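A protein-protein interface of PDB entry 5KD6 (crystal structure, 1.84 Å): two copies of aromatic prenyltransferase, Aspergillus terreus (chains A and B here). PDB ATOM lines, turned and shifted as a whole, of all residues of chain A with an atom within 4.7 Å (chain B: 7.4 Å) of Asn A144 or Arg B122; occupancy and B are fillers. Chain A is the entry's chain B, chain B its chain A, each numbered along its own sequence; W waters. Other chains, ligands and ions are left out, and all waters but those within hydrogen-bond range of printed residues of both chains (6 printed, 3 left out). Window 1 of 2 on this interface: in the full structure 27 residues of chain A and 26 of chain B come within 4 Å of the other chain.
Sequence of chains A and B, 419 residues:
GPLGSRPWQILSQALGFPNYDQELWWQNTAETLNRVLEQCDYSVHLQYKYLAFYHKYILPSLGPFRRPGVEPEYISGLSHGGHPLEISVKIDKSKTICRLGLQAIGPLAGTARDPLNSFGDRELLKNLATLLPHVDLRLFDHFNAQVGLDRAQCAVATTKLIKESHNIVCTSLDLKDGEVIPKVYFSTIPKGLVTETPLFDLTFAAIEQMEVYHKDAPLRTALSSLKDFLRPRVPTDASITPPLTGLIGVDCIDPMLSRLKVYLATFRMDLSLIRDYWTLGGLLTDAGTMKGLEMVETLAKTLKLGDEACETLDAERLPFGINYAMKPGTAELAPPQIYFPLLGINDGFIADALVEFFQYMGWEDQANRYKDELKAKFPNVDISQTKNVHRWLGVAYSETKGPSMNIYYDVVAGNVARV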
ATOM      1  N   ARG A 122       2.601   3.684  21.911  1.00  0.00           N
ATOM      2  CA  ARG A 122       3.032   2.405  21.384  1.00  0.00           C
ATOM      3  C   ARG A 122       1.902   1.350  21.366  1.00  0.00           C
ATOM      4  O   ARG A 122       1.837   0.500  20.425  1.00  0.00           O
ATOM      5  CB  ARG A 122       4.258   1.938  22.162  1.00  0.00           C
ATOM      6  CG  ARG A 122       4.869   0.631  21.729  1.00  0.00           C
ATOM      7  CD  ARG A 122       5.135   0.579  20.254  1.00  0.00           C
ATOM      8  NE  ARG A 122       6.021  -0.552  19.888  1.00  0.00           N
ATOM      9  CZ  ARG A 122       5.705  -1.853  19.955  1.00  0.00           C
ATOM     10  NH1 ARG A 122       4.510  -2.275  20.434  1.00  0.00           N
ATOM     11  NH2 ARG A 122       6.584  -2.741  19.525  1.00  0.00           N
ATOM     12  N   PHE A 140      10.198   3.476  15.831  1.00  0.00           N
ATOM     13  CA  PHE A 140       9.599   3.806  17.100  1.00  0.00           C
ATOM     14  C   PHE A 140      10.371   3.147  18.193  1.00  0.00           C
ATOM     15  O   PHE A 140      10.714   3.762  19.243  1.00  0.00           O
ATOM     16  CB  PHE A 140       8.122   3.351  17.188  1.00  0.00           C
ATOM     17  CG  PHE A 140       7.446   3.811  18.459  1.00  0.00           C
ATOM     18  CD1 PHE A 140       7.728   3.215  19.672  1.00  0.00           C
ATOM     19  CD2 PHE A 140       6.558   4.838  18.428  1.00  0.00           C
ATOM     20  CE1 PHE A 140       7.163   3.647  20.855  1.00  0.00           C
ATOM     21  CE2 PHE A 140       5.967   5.286  19.582  1.00  0.00           C
ATOM     22  CZ  PHE A 140       6.253   4.706  20.802  1.00  0.00           C
ATOM     23  N   ASP A 141      10.534   1.849  18.068  1.00  0.00           N
ATOM     24  CA  ASP A 141      11.149   1.113  19.150  1.00  0.00           C
ATOM     25  C   ASP A 141      12.597   1.581  19.379  1.00  0.00           C
ATOM     26  O   ASP A 141      13.055   1.714  20.495  1.00  0.00           O
ATOM     27  CB  ASP A 141      11.054  -0.377  18.881  1.00  0.00           C
ATOM     28  CG  ASP A 141       9.579  -0.950  19.103  1.00  0.00           C
ATOM     29  OD1 ASP A 141       8.674  -0.279  19.666  1.00  0.00           O
ATOM     30  OD2 ASP A 141       9.346  -2.099  18.707  1.00  0.00           O
ATOM     31  N   HIS A 142      13.291   1.843  18.313  1.00  0.00           N
ATOM     32  CA  HIS A 142      14.666   2.268  18.414  1.00  0.00           C
ATOM     33  C   HIS A 142      14.747   3.562  19.238  1.00  0.00           C
ATOM     34  O   HIS A 142      15.479   3.622  20.245  1.00  0.00           O
ATOM     35  CB  HIS A 142      15.266   2.532  17.048  1.00  0.00           C
ATOM     36  CG  HIS A 142      16.589   3.206  17.147  1.00  0.00           C
ATOM     37  ND1 HIS A 142      17.717   2.519  17.520  1.00  0.00           N
ATOM     38  CD2 HIS A 142      16.944   4.509  17.084  1.00  0.00           C
ATOM     39  CE1 HIS A 142      18.738   3.350  17.600  1.00  0.00           C
ATOM     40  NE2 HIS A 142      18.295   4.570  17.365  1.00  0.00           N
ATOM     41  N   PHE A 143      13.943   4.565  18.872  1.00  0.00           N
ATOM     42  CA  PHE A 143      14.002   5.837  19.579  1.00  0.00           C
ATOM     43  C   PHE A 143      13.370   5.787  20.963  1.00  0.00           C
ATOM     44  O   PHE A 143      13.861   6.393  21.875  1.00  0.00           O
ATOM     45  CB  PHE A 143      13.458   6.982  18.693  1.00  0.00           C
ATOM     46  CG  PHE A 143      14.412   7.413  17.665  1.00  0.00           C
ATOM     47  CD1 PHE A 143      15.530   8.146  18.022  1.00  0.00           C
ATOM     48  CD2 PHE A 143      14.278   7.009  16.379  1.00  0.00           C
ATOM     49  CE1 PHE A 143      16.480   8.470  17.061  1.00  0.00           C
ATOM     50  CE2 PHE A 143      15.205   7.360  15.411  1.00  0.00           C
ATOM     51  CZ  PHE A 143      16.317   8.101  15.762  1.00  0.00           C
ATOM     52  N   ASN A 144      12.324   5.005  21.146  1.00  0.00           N
ATOM     53  CA  ASN A 144      11.822   4.744  22.465  1.00  0.00           C
ATOM     54  C   ASN A 144      12.874   4.153  23.394  1.00  0.00           C
ATOM     55  O   ASN A 144      12.916   4.485  24.588  1.00  0.00           O
ATOM     56  CB  ASN A 144      10.601   3.801  22.418  1.00  0.00           C
ATOM     57  CG  ASN A 144       9.698   3.951  23.614  1.00  0.00           C
ATOM     58  OD1 ASN A 144       9.182   2.968  24.155  1.00  0.00           O
ATOM     59  ND2 ASN A 144       9.474   5.168  24.027  1.00  0.00           N
ATOM     60  N   ALA A 145      13.697   3.254  22.878  1.00  0.00           N
ATOM     61  CA  ALA A 145      14.819   2.720  23.675  1.00  0.00           C
ATOM     62  C   ALA A 145      15.864   3.802  24.016  1.00  0.00           C
ATOM     63  O   ALA A 145      16.408   3.843  25.154  1.00  0.00           O
ATOM     64  CB  ALA A 145      15.489   1.539  22.964  1.00  0.00           C
ATOM     65  N   GLN A 146      16.101   4.704  23.093  1.00  0.00           N
ATOM     66  CA  GLN A 146      17.176   5.706  23.275  1.00  0.00           C
ATOM     67  C   GLN A 146      16.762   6.887  24.123  1.00  0.00           C
ATOM     68  O   GLN A 146      17.599   7.450  24.844  1.00  0.00           O
ATOM     69  CB  GLN A 146      17.652   6.258  21.927  1.00  0.00           C
ATOM     70  CG  GLN A 146      18.048   5.255  20.886  1.00  0.00           C
ATOM     71  CD  GLN A 146      18.945   4.188  21.367  1.00  0.00           C
ATOM     72  OE1 GLN A 146      18.657   2.969  21.229  1.00  0.00           O
ATOM     73  NE2 GLN A 146      20.064   4.613  21.914  1.00  0.00           N
ATOM     74  N   VAL A 147      15.509   7.314  24.049  1.00  0.00           N
ATOM     75  CA  VAL A 147      15.091   8.492  24.822  1.00  0.00           C
ATOM     76  C   VAL A 147      13.985   8.231  25.852  1.00  0.00           C
ATOM     77  O   VAL A 147      13.641   9.147  26.616  1.00  0.00           O
ATOM     78  CB  VAL A 147      14.739   9.688  23.915  1.00  0.00           C
ATOM     79  CG1 VAL A 147      15.811   9.936  22.885  1.00  0.00           C
ATOM     80  CG2 VAL A 147      13.362   9.526  23.280  1.00  0.00           C
ATOM     81  N   GLY A 148      13.459   6.995  25.938  1.00  0.00           N
ATOM     82  CA  GLY A 148      12.511   6.647  26.986  1.00  0.00           C
ATOM     83  C   GLY A 148      13.207   6.652  28.358  1.00  0.00           C
ATOM     84  O   GLY A 148      14.430   6.573  28.458  1.00  0.00           O
ATOM     85  N   ILE A 168       6.744  12.236  26.426  1.00  0.00           N
ATOM     86  CA  ILE A 168       7.914  11.615  25.826  1.00  0.00           C
ATOM     87  C   ILE A 168       7.665  11.435  24.321  1.00  0.00           C
ATOM     88  O   ILE A 168       8.606  11.492  23.540  1.00  0.00           O
ATOM     89  CB  ILE A 168       8.260  10.233  26.476  1.00  0.00           C
ATOM     90  CG1 ILE A 168       9.045  10.399  27.780  1.00  0.00           C
ATOM     91  CG2 ILE A 168       9.172   9.371  25.596  1.00  0.00           C
ATOM     92  CD1 ILE A 168      10.510  10.737  27.566  1.00  0.00           C
ATOM     93  N   PHE A 186       9.556  12.130  19.288  1.00  0.00           N
ATOM     94  CA  PHE A 186      10.059  11.862  20.579  1.00  0.00           C
ATOM     95  C   PHE A 186      10.696  13.076  21.174  1.00  0.00           C
ATOM     96  O   PHE A 186      11.551  13.747  20.507  1.00  0.00           O
ATOM     97  CB  PHE A 186      11.148  10.769  20.448  1.00  0.00           C
ATOM     98  CG  PHE A 186      10.595   9.408  20.206  1.00  0.00           C
ATOM     99  CD1 PHE A 186      10.153   8.655  21.262  1.00  0.00           C
ATOM    100  CD2 PHE A 186      10.473   8.897  18.924  1.00  0.00           C
ATOM    101  CE1 PHE A 186       9.625   7.394  21.028  1.00  0.00           C
ATOM    102  CE2 PHE A 186       9.875   7.653  18.692  1.00  0.00           C
ATOM    103  CZ  PHE A 186       9.461   6.908  19.758  1.00  0.00           C
ATOM    104  N   ALA B 104       3.672 -14.596  25.110  1.00  0.00           N
ATOM    105  CA  ALA B 104       2.455 -13.892  25.267  1.00  0.00           C
ATOM    106  C   ALA B 104       1.749 -13.847  23.901  1.00  0.00           C
ATOM    107  O   ALA B 104       2.287 -13.267  22.948  1.00  0.00           O
ATOM    108  CB  ALA B 104       2.713 -12.508  25.815  1.00  0.00           C
ATOM    109  N   ASN B 117       3.747 -13.715  15.854  1.00  0.00           N
ATOM    110  CA  ASN B 117       3.370 -13.268  17.217  1.00  0.00           C
ATOM    111  C   ASN B 117       4.280 -12.166  17.746  1.00  0.00           C
ATOM    112  O   ASN B 117       4.975 -12.304  18.784  1.00  0.00           O
ATOM    113  CB  ASN B 117       3.328 -14.452  18.206  1.00  0.00           C
ATOM    114  CG  ASN B 117       2.696 -14.052  19.517  1.00  0.00           C
ATOM    115  OD1 ASN B 117       1.626 -13.471  19.550  1.00  0.00           O
ATOM    116  ND2 ASN B 117       3.468 -14.189  20.589  1.00  0.00           N
ATOM    117  N   SER B 118       4.295 -11.076  17.028  1.00  0.00           N
ATOM    118  CA  SER B 118       5.267 -10.023  17.226  1.00  0.00           C
ATOM    119  C   SER B 118       4.908  -8.979  18.303  1.00  0.00           C
ATOM    120  O   SER B 118       5.702  -8.114  18.537  1.00  0.00           O
ATOM    121  CB  SER B 118       5.506  -9.281  15.895  1.00  0.00           C
ATOM    122  OG  SER B 118       6.160 -10.181  14.992  1.00  0.00           O
ATOM    123  N   PHE B 119       3.704  -9.038  18.866  1.00  0.00           N
ATOM    124  CA  PHE B 119       3.161  -7.904  19.673  1.00  0.00           C
ATOM    125  C   PHE B 119       2.806  -8.278  21.093  1.00  0.00           C
ATOM    126  O   PHE B 119       2.795  -7.372  21.963  1.00  0.00           O
ATOM    127  CB  PHE B 119       1.906  -7.302  19.017  1.00  0.00           C
ATOM    128  CG  PHE B 119       2.124  -6.953  17.583  1.00  0.00           C
ATOM    129  CD1 PHE B 119       2.979  -5.927  17.273  1.00  0.00           C
ATOM    130  CD2 PHE B 119       1.596  -7.731  16.584  1.00  0.00           C
ATOM    131  CE1 PHE B 119       3.273  -5.613  15.947  1.00  0.00           C
ATOM    132  CE2 PHE B 119       1.897  -7.449  15.235  1.00  0.00           C
ATOM    133  CZ  PHE B 119       2.752  -6.394  14.925  1.00  0.00           C
ATOM    134  N   GLY B 120       2.472  -9.551  21.336  1.00  0.00           N
ATOM    135  CA  GLY B 120       1.869  -9.909  22.621  1.00  0.00           C
ATOM    136  C   GLY B 120       2.840  -9.705  23.791  1.00  0.00           C
ATOM    137  O   GLY B 120       2.433  -9.287  24.871  1.00  0.00           O
ATOM    138  N   ASP B 121       4.112 -10.030  23.610  1.00  0.00           N
ATOM    139  CA  ASP B 121       5.054  -9.944  24.723  1.00  0.00           C
ATOM    140  C   ASP B 121       5.291  -8.480  25.198  1.00  0.00           C
ATOM    141  O   ASP B 121       5.347  -8.238  26.400  1.00  0.00           O
ATOM    142  CB  ASP B 121       6.389 -10.666  24.404  1.00  0.00           C
ATOM    143  CG  ASP B 121       6.222 -12.234  24.323  1.00  0.00           C
ATOM    144  OD1 ASP B 121       5.839 -12.804  23.249  1.00  0.00           O
ATOM    145  OD2 ASP B 121       6.445 -12.909  25.367  1.00  0.00           O
ATOM    146  N   ARG B 122       5.432  -7.571  24.254  1.00  0.00           N
ATOM    147  CA  ARG B 122       5.537  -6.158  24.563  1.00  0.00           C
ATOM    148  C   ARG B 122       4.263  -5.654  25.274  1.00  0.00           C
ATOM    149  O   ARG B 122       4.385  -4.898  26.230  1.00  0.00           O
ATOM    150  CB  ARG B 122       5.901  -5.381  23.325  1.00  0.00           C
ATOM    151  CG  ARG B 122       6.197  -3.871  23.465  1.00  0.00           C
ATOM    152  CD  ARG B 122       7.136  -3.526  24.567  1.00  0.00           C
ATOM    153  NE  ARG B 122       7.633  -2.118  24.538  1.00  0.00           N
ATOM    154  CZ  ARG B 122       6.926  -1.011  24.815  1.00  0.00           C
ATOM    155  NH1 ARG B 122       5.613  -1.070  25.092  1.00  0.00           N
ATOM    156  NH2 ARG B 122       7.551   0.161  24.881  1.00  0.00           N
ATOM    157  N   GLU B 123       3.086  -6.115  24.851  1.00  0.00           N
ATOM    158  CA  GLU B 123       1.847  -5.784  25.512  1.00  0.00           C
ATOM    159  C   GLU B 123       1.857  -6.225  26.977  1.00  0.00           C
ATOM    160  O   GLU B 123       1.450  -5.457  27.884  1.00  0.00           O
ATOM    161  CB  GLU B 123       0.598  -6.282  24.771  1.00  0.00           C
ATOM    162  CG  GLU B 123      -0.694  -6.046  25.571  1.00  0.00           C
ATOM    163  CD  GLU B 123      -2.009  -6.146  24.830  1.00  0.00           C
ATOM    164  OE1 GLU B 123      -2.051  -6.478  23.627  1.00  0.00           O
ATOM    165  OE2 GLU B 123      -3.027  -5.810  25.470  1.00  0.00           O
ATOM    166  N   LEU B 124       2.294  -7.454  27.190  1.00  0.00           N
ATOM    167  CA  LEU B 124       2.424  -7.925  28.584  1.00  0.00           C
ATOM    168  C   LEU B 124       3.422  -7.062  29.363  1.00  0.00           C
ATOM    169  O   LEU B 124       3.204  -6.636  30.505  1.00  0.00           O
ATOM    170  CB  LEU B 124       2.890  -9.403  28.582  1.00  0.00           C
ATOM    171  CG  LEU B 124       3.243  -9.988  29.962  1.00  0.00           C
ATOM    172  CD1 LEU B 124       2.098  -9.911  30.940  1.00  0.00           C
ATOM    173  CD2 LEU B 124       3.723 -11.429  29.751  1.00  0.00           C
ATOM    174  N   LEU B 125       4.571  -6.833  28.769  1.00  0.00           N
ATOM    175  CA  LEU B 125       5.608  -6.050  29.441  1.00  0.00           C
ATOM    176  C   LEU B 125       5.129  -4.633  29.768  1.00  0.00           C
ATOM    177  O   LEU B 125       5.471  -4.115  30.857  1.00  0.00           O
ATOM    178  CB  LEU B 125       6.833  -6.021  28.567  1.00  0.00           C
ATOM    179  CG  LEU B 125       7.706  -7.223  28.928  1.00  0.00           C
ATOM    180  CD1 LEU B 125       8.605  -7.622  27.776  1.00  0.00           C
ATOM    181  CD2 LEU B 125       8.497  -6.785  30.182  1.00  0.00           C
ATOM    182  N   LYS B 126       4.317  -4.061  28.882  1.00  0.00           N
ATOM    183  CA  LYS B 126       3.700  -2.697  29.134  1.00  0.00           C
ATOM    184  C   LYS B 126       2.842  -2.732  30.413  1.00  0.00           C
ATOM    185  O   LYS B 126       2.964  -1.886  31.302  1.00  0.00           O
ATOM    186  CB  LYS B 126       2.829  -2.234  27.965  1.00  0.00           C
ATOM    187  CG  LYS B 126       2.015  -0.975  28.261  1.00  0.00           C
ATOM    188  CD  LYS B 126       0.751  -0.888  27.435  1.00  0.00           C
ATOM    189  CE  LYS B 126      -0.369  -1.731  27.990  1.00  0.00           C
ATOM    190  NZ  LYS B 126      -1.417  -1.823  26.938  1.00  0.00           N
ATOM    191  N   ASN B 127       2.021  -3.767  30.513  1.00  0.00           N
ATOM    192  CA  ASN B 127       1.249  -4.000  31.713  1.00  0.00           C
ATOM    193  C   ASN B 127       2.050  -4.289  32.937  1.00  0.00           C
ATOM    194  O   ASN B 127       1.694  -3.791  34.036  1.00  0.00           O
ATOM    195  CB  ASN B 127       0.122  -4.989  31.462  1.00  0.00           C
ATOM    196  CG  ASN B 127      -0.877  -4.435  30.484  1.00  0.00           C
ATOM    197  OD1 ASN B 127      -1.163  -3.204  30.495  1.00  0.00           O
ATOM    198  ND2 ASN B 127      -1.292  -5.241  29.588  1.00  0.00           N
ATOM    199  N   LEU B 128       3.189  -4.958  32.771  1.00  0.00           N
ATOM    200  CA  LEU B 128       4.103  -5.103  33.869  1.00  0.00           C
ATOM    201  C   LEU B 128       4.806  -3.828  34.300  1.00  0.00           C
ATOM    202  O   LEU B 128       5.078  -3.629  35.527  1.00  0.00           O
ATOM    203  CB  LEU B 128       5.108  -6.237  33.566  1.00  0.00           C
ATOM    204  CG  LEU B 128       4.515  -7.612  33.284  1.00  0.00           C
ATOM    205  CD1 LEU B 128       5.704  -8.586  33.180  1.00  0.00           C
ATOM    206  CD2 LEU B 128       3.567  -8.002  34.360  1.00  0.00           C
ATOM    207  N   ALA B 129       5.066  -2.932  33.349  1.00  0.00           N
ATOM    208  CA  ALA B 129       5.650  -1.639  33.662  1.00  0.00           C
ATOM    209  C   ALA B 129       4.756  -0.694  34.492  1.00  0.00           C
ATOM    210  O   ALA B 129       5.301   0.116  35.199  1.00  0.00           O
ATOM    211  CB  ALA B 129       6.084  -0.914  32.392  1.00  0.00           C
ATOM    212  N   LEU B 137      11.660  -1.122  29.917  1.00  0.00           N
ATOM    213  CA  LEU B 137      11.391  -1.586  28.557  1.00  0.00           C
ATOM    214  C   LEU B 137      12.464  -1.243  27.541  1.00  0.00           C
ATOM    215  O   LEU B 137      12.368  -1.651  26.382  1.00  0.00           O
ATOM    216  CB  LEU B 137      10.054  -1.011  28.077  1.00  0.00           C
ATOM    217  CG  LEU B 137       8.839  -1.359  28.965  1.00  0.00           C
ATOM    218  CD1 LEU B 137       7.595  -1.117  28.159  1.00  0.00           C
ATOM    219  CD2 LEU B 137       8.837  -2.798  29.429  1.00  0.00           C
ATOM    220  N   ARG B 138      13.526  -0.587  27.959  1.00  0.00           N
ATOM    221  CA  ARG B 138      14.477  -0.008  26.962  1.00  0.00           C
ATOM    222  C   ARG B 138      15.279  -1.047  26.244  1.00  0.00           C
ATOM    223  O   ARG B 138      15.419  -0.978  25.049  1.00  0.00           O
ATOM    224  CB  ARG B 138      15.353   1.040  27.598  1.00  0.00           C
ATOM    225  CG  ARG B 138      14.601   2.327  27.892  1.00  0.00           C
ATOM    226  CD  ARG B 138      15.425   3.315  28.647  1.00  0.00           C
ATOM    227  NE  ARG B 138      15.591   2.900  30.057  1.00  0.00           N
ATOM    228  CZ  ARG B 138      15.944   3.726  31.049  1.00  0.00           C
ATOM    229  NH1 ARG B 138      16.077   5.030  30.835  1.00  0.00           N
ATOM    230  NH2 ARG B 138      16.074   3.256  32.266  1.00  0.00           N
ATOM    231  N   PHE B 140      14.286  -4.293  25.877  1.00  0.00           N
ATOM    232  CA  PHE B 140      13.267  -4.908  25.032  1.00  0.00           C
ATOM    233  C   PHE B 140      13.141  -4.127  23.715  1.00  0.00           C
ATOM    234  O   PHE B 140      13.233  -4.680  22.578  1.00  0.00           O
ATOM    235  CB  PHE B 140      11.932  -5.018  25.731  1.00  0.00           C
ATOM    236  CG  PHE B 140      10.908  -5.711  24.890  1.00  0.00           C
ATOM    237  CD1 PHE B 140      10.393  -5.096  23.775  1.00  0.00           C
ATOM    238  CD2 PHE B 140      10.593  -7.010  25.125  1.00  0.00           C
ATOM    239  CE1 PHE B 140       9.491  -5.756  22.914  1.00  0.00           C
ATOM    240  CE2 PHE B 140       9.665  -7.666  24.341  1.00  0.00           C
ATOM    241  CZ  PHE B 140       9.142  -7.064  23.220  1.00  0.00           C
ATOM    242  N   ASP B 141      12.898  -2.845  23.848  1.00  0.00           N
ATOM    243  CA  ASP B 141      12.699  -2.031  22.674  1.00  0.00           C
ATOM    244  C   ASP B 141      13.872  -1.957  21.739  1.00  0.00           C
ATOM    245  O   ASP B 141      13.721  -1.980  20.515  1.00  0.00           O
ATOM    246  CB  ASP B 141      12.229  -0.643  23.069  1.00  0.00           C
ATOM    247  CG  ASP B 141      10.771  -0.633  23.594  1.00  0.00           C
ATOM    248  OD1 ASP B 141       9.997  -1.568  23.309  1.00  0.00           O
ATOM    249  OD2 ASP B 141      10.373   0.347  24.301  1.00  0.00           O
ATOM    250  N   HIS B 142      15.083  -1.914  22.313  1.00  0.00           N
ATOM    251  CA  HIS B 142      16.243  -1.962  21.501  1.00  0.00           C
ATOM    252  C   HIS B 142      16.346  -3.228  20.608  1.00  0.00           C
ATOM    253  O   HIS B 142      16.522  -3.121  19.398  1.00  0.00           O
ATOM    254  CB  HIS B 142      17.503  -1.883  22.380  1.00  0.00           C
ATOM    255  CG  HIS B 142      18.746  -2.055  21.575  1.00  0.00           C
ATOM    256  ND1 HIS B 142      19.234  -1.056  20.757  1.00  0.00           N
ATOM    257  CD2 HIS B 142      19.475  -3.147  21.309  1.00  0.00           C
ATOM    258  CE1 HIS B 142      20.263  -1.518  20.086  1.00  0.00           C
ATOM    259  NE2 HIS B 142      20.424  -2.784  20.397  1.00  0.00           N
ATOM    260  N   ASN B 144      13.964  -5.398  20.016  1.00  0.00           N
ATOM    261  CA  ASN B 144      12.804  -5.466  19.112  1.00  0.00           C
ATOM    262  C   ASN B 144      13.065  -4.674  17.852  1.00  0.00           C
ATOM    263  O   ASN B 144      12.680  -5.139  16.735  1.00  0.00           O
ATOM    264  CB  ASN B 144      11.527  -5.035  19.803  1.00  0.00           C
ATOM    265  CG  ASN B 144      10.293  -5.688  19.205  1.00  0.00           C
ATOM    266  OD1 ASN B 144      10.302  -6.839  18.826  1.00  0.00           O
ATOM    267  ND2 ASN B 144       9.239  -4.945  19.139  1.00  0.00           N
ATOM    268  N   VAL B 169      10.176 -13.556  19.985  1.00  0.00           N
ATOM    269  CA  VAL B 169      10.512 -13.247  21.398  1.00  0.00           C
ATOM    270  C   VAL B 169       9.788 -14.196  22.287  1.00  0.00           C
ATOM    271  O   VAL B 169       8.742 -14.773  21.927  1.00  0.00           O
ATOM    272  CB  VAL B 169      10.245 -11.722  21.696  1.00  0.00           C
ATOM    273  CG1 VAL B 169       8.839 -11.409  21.606  1.00  0.00           C
ATOM    274  CG2 VAL B 169      10.781 -11.250  23.050  1.00  0.00           C
ATOM    275  N   THR B 171       9.334 -14.648  26.909  1.00  0.00           N
ATOM    276  CA  THR B 171       9.449 -13.889  28.169  1.00  0.00           C
ATOM    277  C   THR B 171       9.650 -14.868  29.317  1.00  0.00           C
ATOM    278  O   THR B 171       9.071 -15.923  29.275  1.00  0.00           O
ATOM    279  CB  THR B 171       8.163 -13.070  28.371  1.00  0.00           C
ATOM    280  OG1 THR B 171       8.044 -12.116  27.318  1.00  0.00           O
ATOM    281  CG2 THR B 171       8.169 -12.342  29.715  1.00  0.00           C
ATOM    282  N   VAL B 184      13.605 -11.243  28.801  1.00  0.00           N
ATOM    283  CA  VAL B 184      13.180 -11.662  27.478  1.00  0.00           C
ATOM    284  C   VAL B 184      14.313 -12.241  26.666  1.00  0.00           C
ATOM    285  O   VAL B 184      15.524 -11.998  26.947  1.00  0.00           O
ATOM    286  CB  VAL B 184      12.533 -10.518  26.721  1.00  0.00           C
ATOM    287  CG1 VAL B 184      11.240 -10.112  27.441  1.00  0.00           C
ATOM    288  CG2 VAL B 184      13.493  -9.373  26.568  1.00  0.00           C
HETATM  289  O   HOH W   1       3.124  -4.690  21.418  1.00  0.00           O
HETATM  290  O   HOH W   2       9.089  -2.948  21.382  1.00  0.00           O
HETATM  291  O   HOH W   3       7.148   2.613  26.439  1.00  0.00           O
HETATM  292  O   HOH W   4      11.820   1.989  25.948  1.00  0.00           O
HETATM  293  O   HOH W   5      20.008   0.959  23.145  1.00  0.00           O
HETATM  294  O   HOH W   6      10.138  -3.194  16.290  1.00  0.00           O
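Among the printed residues, pairs that only touch across the chains: Ala A145 with Arg B138, Asp A141 with Asp B141, Ala A145 with His B142, Arg A122 with Arg B122 and Ala A145 with Asp B141.
OD1 of Asp A141 is in salt-bridge range of NE of Arg A122 (2.7 Å). The side-chain carboxylate (OD1) of Asp B141 is in salt-bridge range of the guanidinium group (NE) of Arg B122 (2.7 Å).
Water W2 lies within hydrogen-bond range of OD1 of Asp B141, OD2 of Asp A141, ND2 of Asn B144 and NH2 of Arg A122. Water W4 lies within hydrogen-bond range of the side-chain carboxylate (OD2) of Asp B141 and the backbone carbonyl oxygen (O) of Asn A144. Water W1 lies within hydrogen-bond range of the backbone carbonyl oxygen of Phe B119 (2.8 Å) and the guanidinium group of Arg A122 (3.0 Å). Water W6 bridges OD2 of Asp A141 (2.8 Å) and O of Asn B144 (3.2 Å). Water W3 lies within hydrogen-bond range of the guanidinium group of Arg B122 and the side-chain amide oxygen of Asn A144. Water W5 bridges OE1 of Gln A146 and ND1 of His B142.
Of the printed residues of chain B, Asn A144 touches Arg B122 and Asp B141. Printed residues of chain B within 4 Å of Asp A141: Asp B141 and Asn B144. Printed residues of chain A within 4 Å of Arg B138: Ala A145 (3.3 Å) and Gly A148 (3.3 Å). Of the printed residues of chain B, Gly A148 touches Arg B138 (3.3 Å). Printed residues of chain B within 4 Å of Ala A145: Arg B138, Asp B141 and His B142. The nearest printed residue of chain A that does not touch Arg B122 is Asp A141 (5.3 Å).
The side-chain amide nitrogen (ND2) of Asn B144 is in hydrogen-bond range of the side-chain carboxylate (OD2) of Asp A141, at 2.9 Å. The guanidinium group of Arg A122 sits close to the side-chain amide nitrogen of Asn B144, 3.5 Å away. OD1 of Asn A144 sits at hydrogen-bond distance from NH2 of Arg B122 (3.3 Å). The side-chain carboxylate of Asp B141 lies close to the side-chain amide oxygen of Asn A144, at 2.9 Å. The backbone carbonyl oxygen (O) of Gly A148 sits at hydrogen-bond distance from the guanidinium group (NH1) of Arg B138, 3.3 Å away.
Of the 12 printed residues of chain A, 5 touch a printed residue of chain B. Hydrophobic or aromatic side chains of chain A that line the printed part of chain B: Ala A145. Among the printed residues, 10 pairs touch across the chains. Among the printed residues, no Asp or Glu carboxylate lies within 4 Å of a Lys or Arg side-chain nitrogen of the other chain.
Arg A122 touches its own counterpart, Arg B122. Arg A122 touches Asn B144, and with the chains exchanged Asn A144 touches Arg B122. Asp B141 touches its own counterpart, Asp A141. Asp A141 touches Asn B144, and with the chains exchanged Asn A144 touches Asp B141. Positions printed for both chains: 122, 140, 141, 142 and 144. Of the 10 pairs that touch across the chains among the printed residues, 6 have their exchanged pair printed and touching as well.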
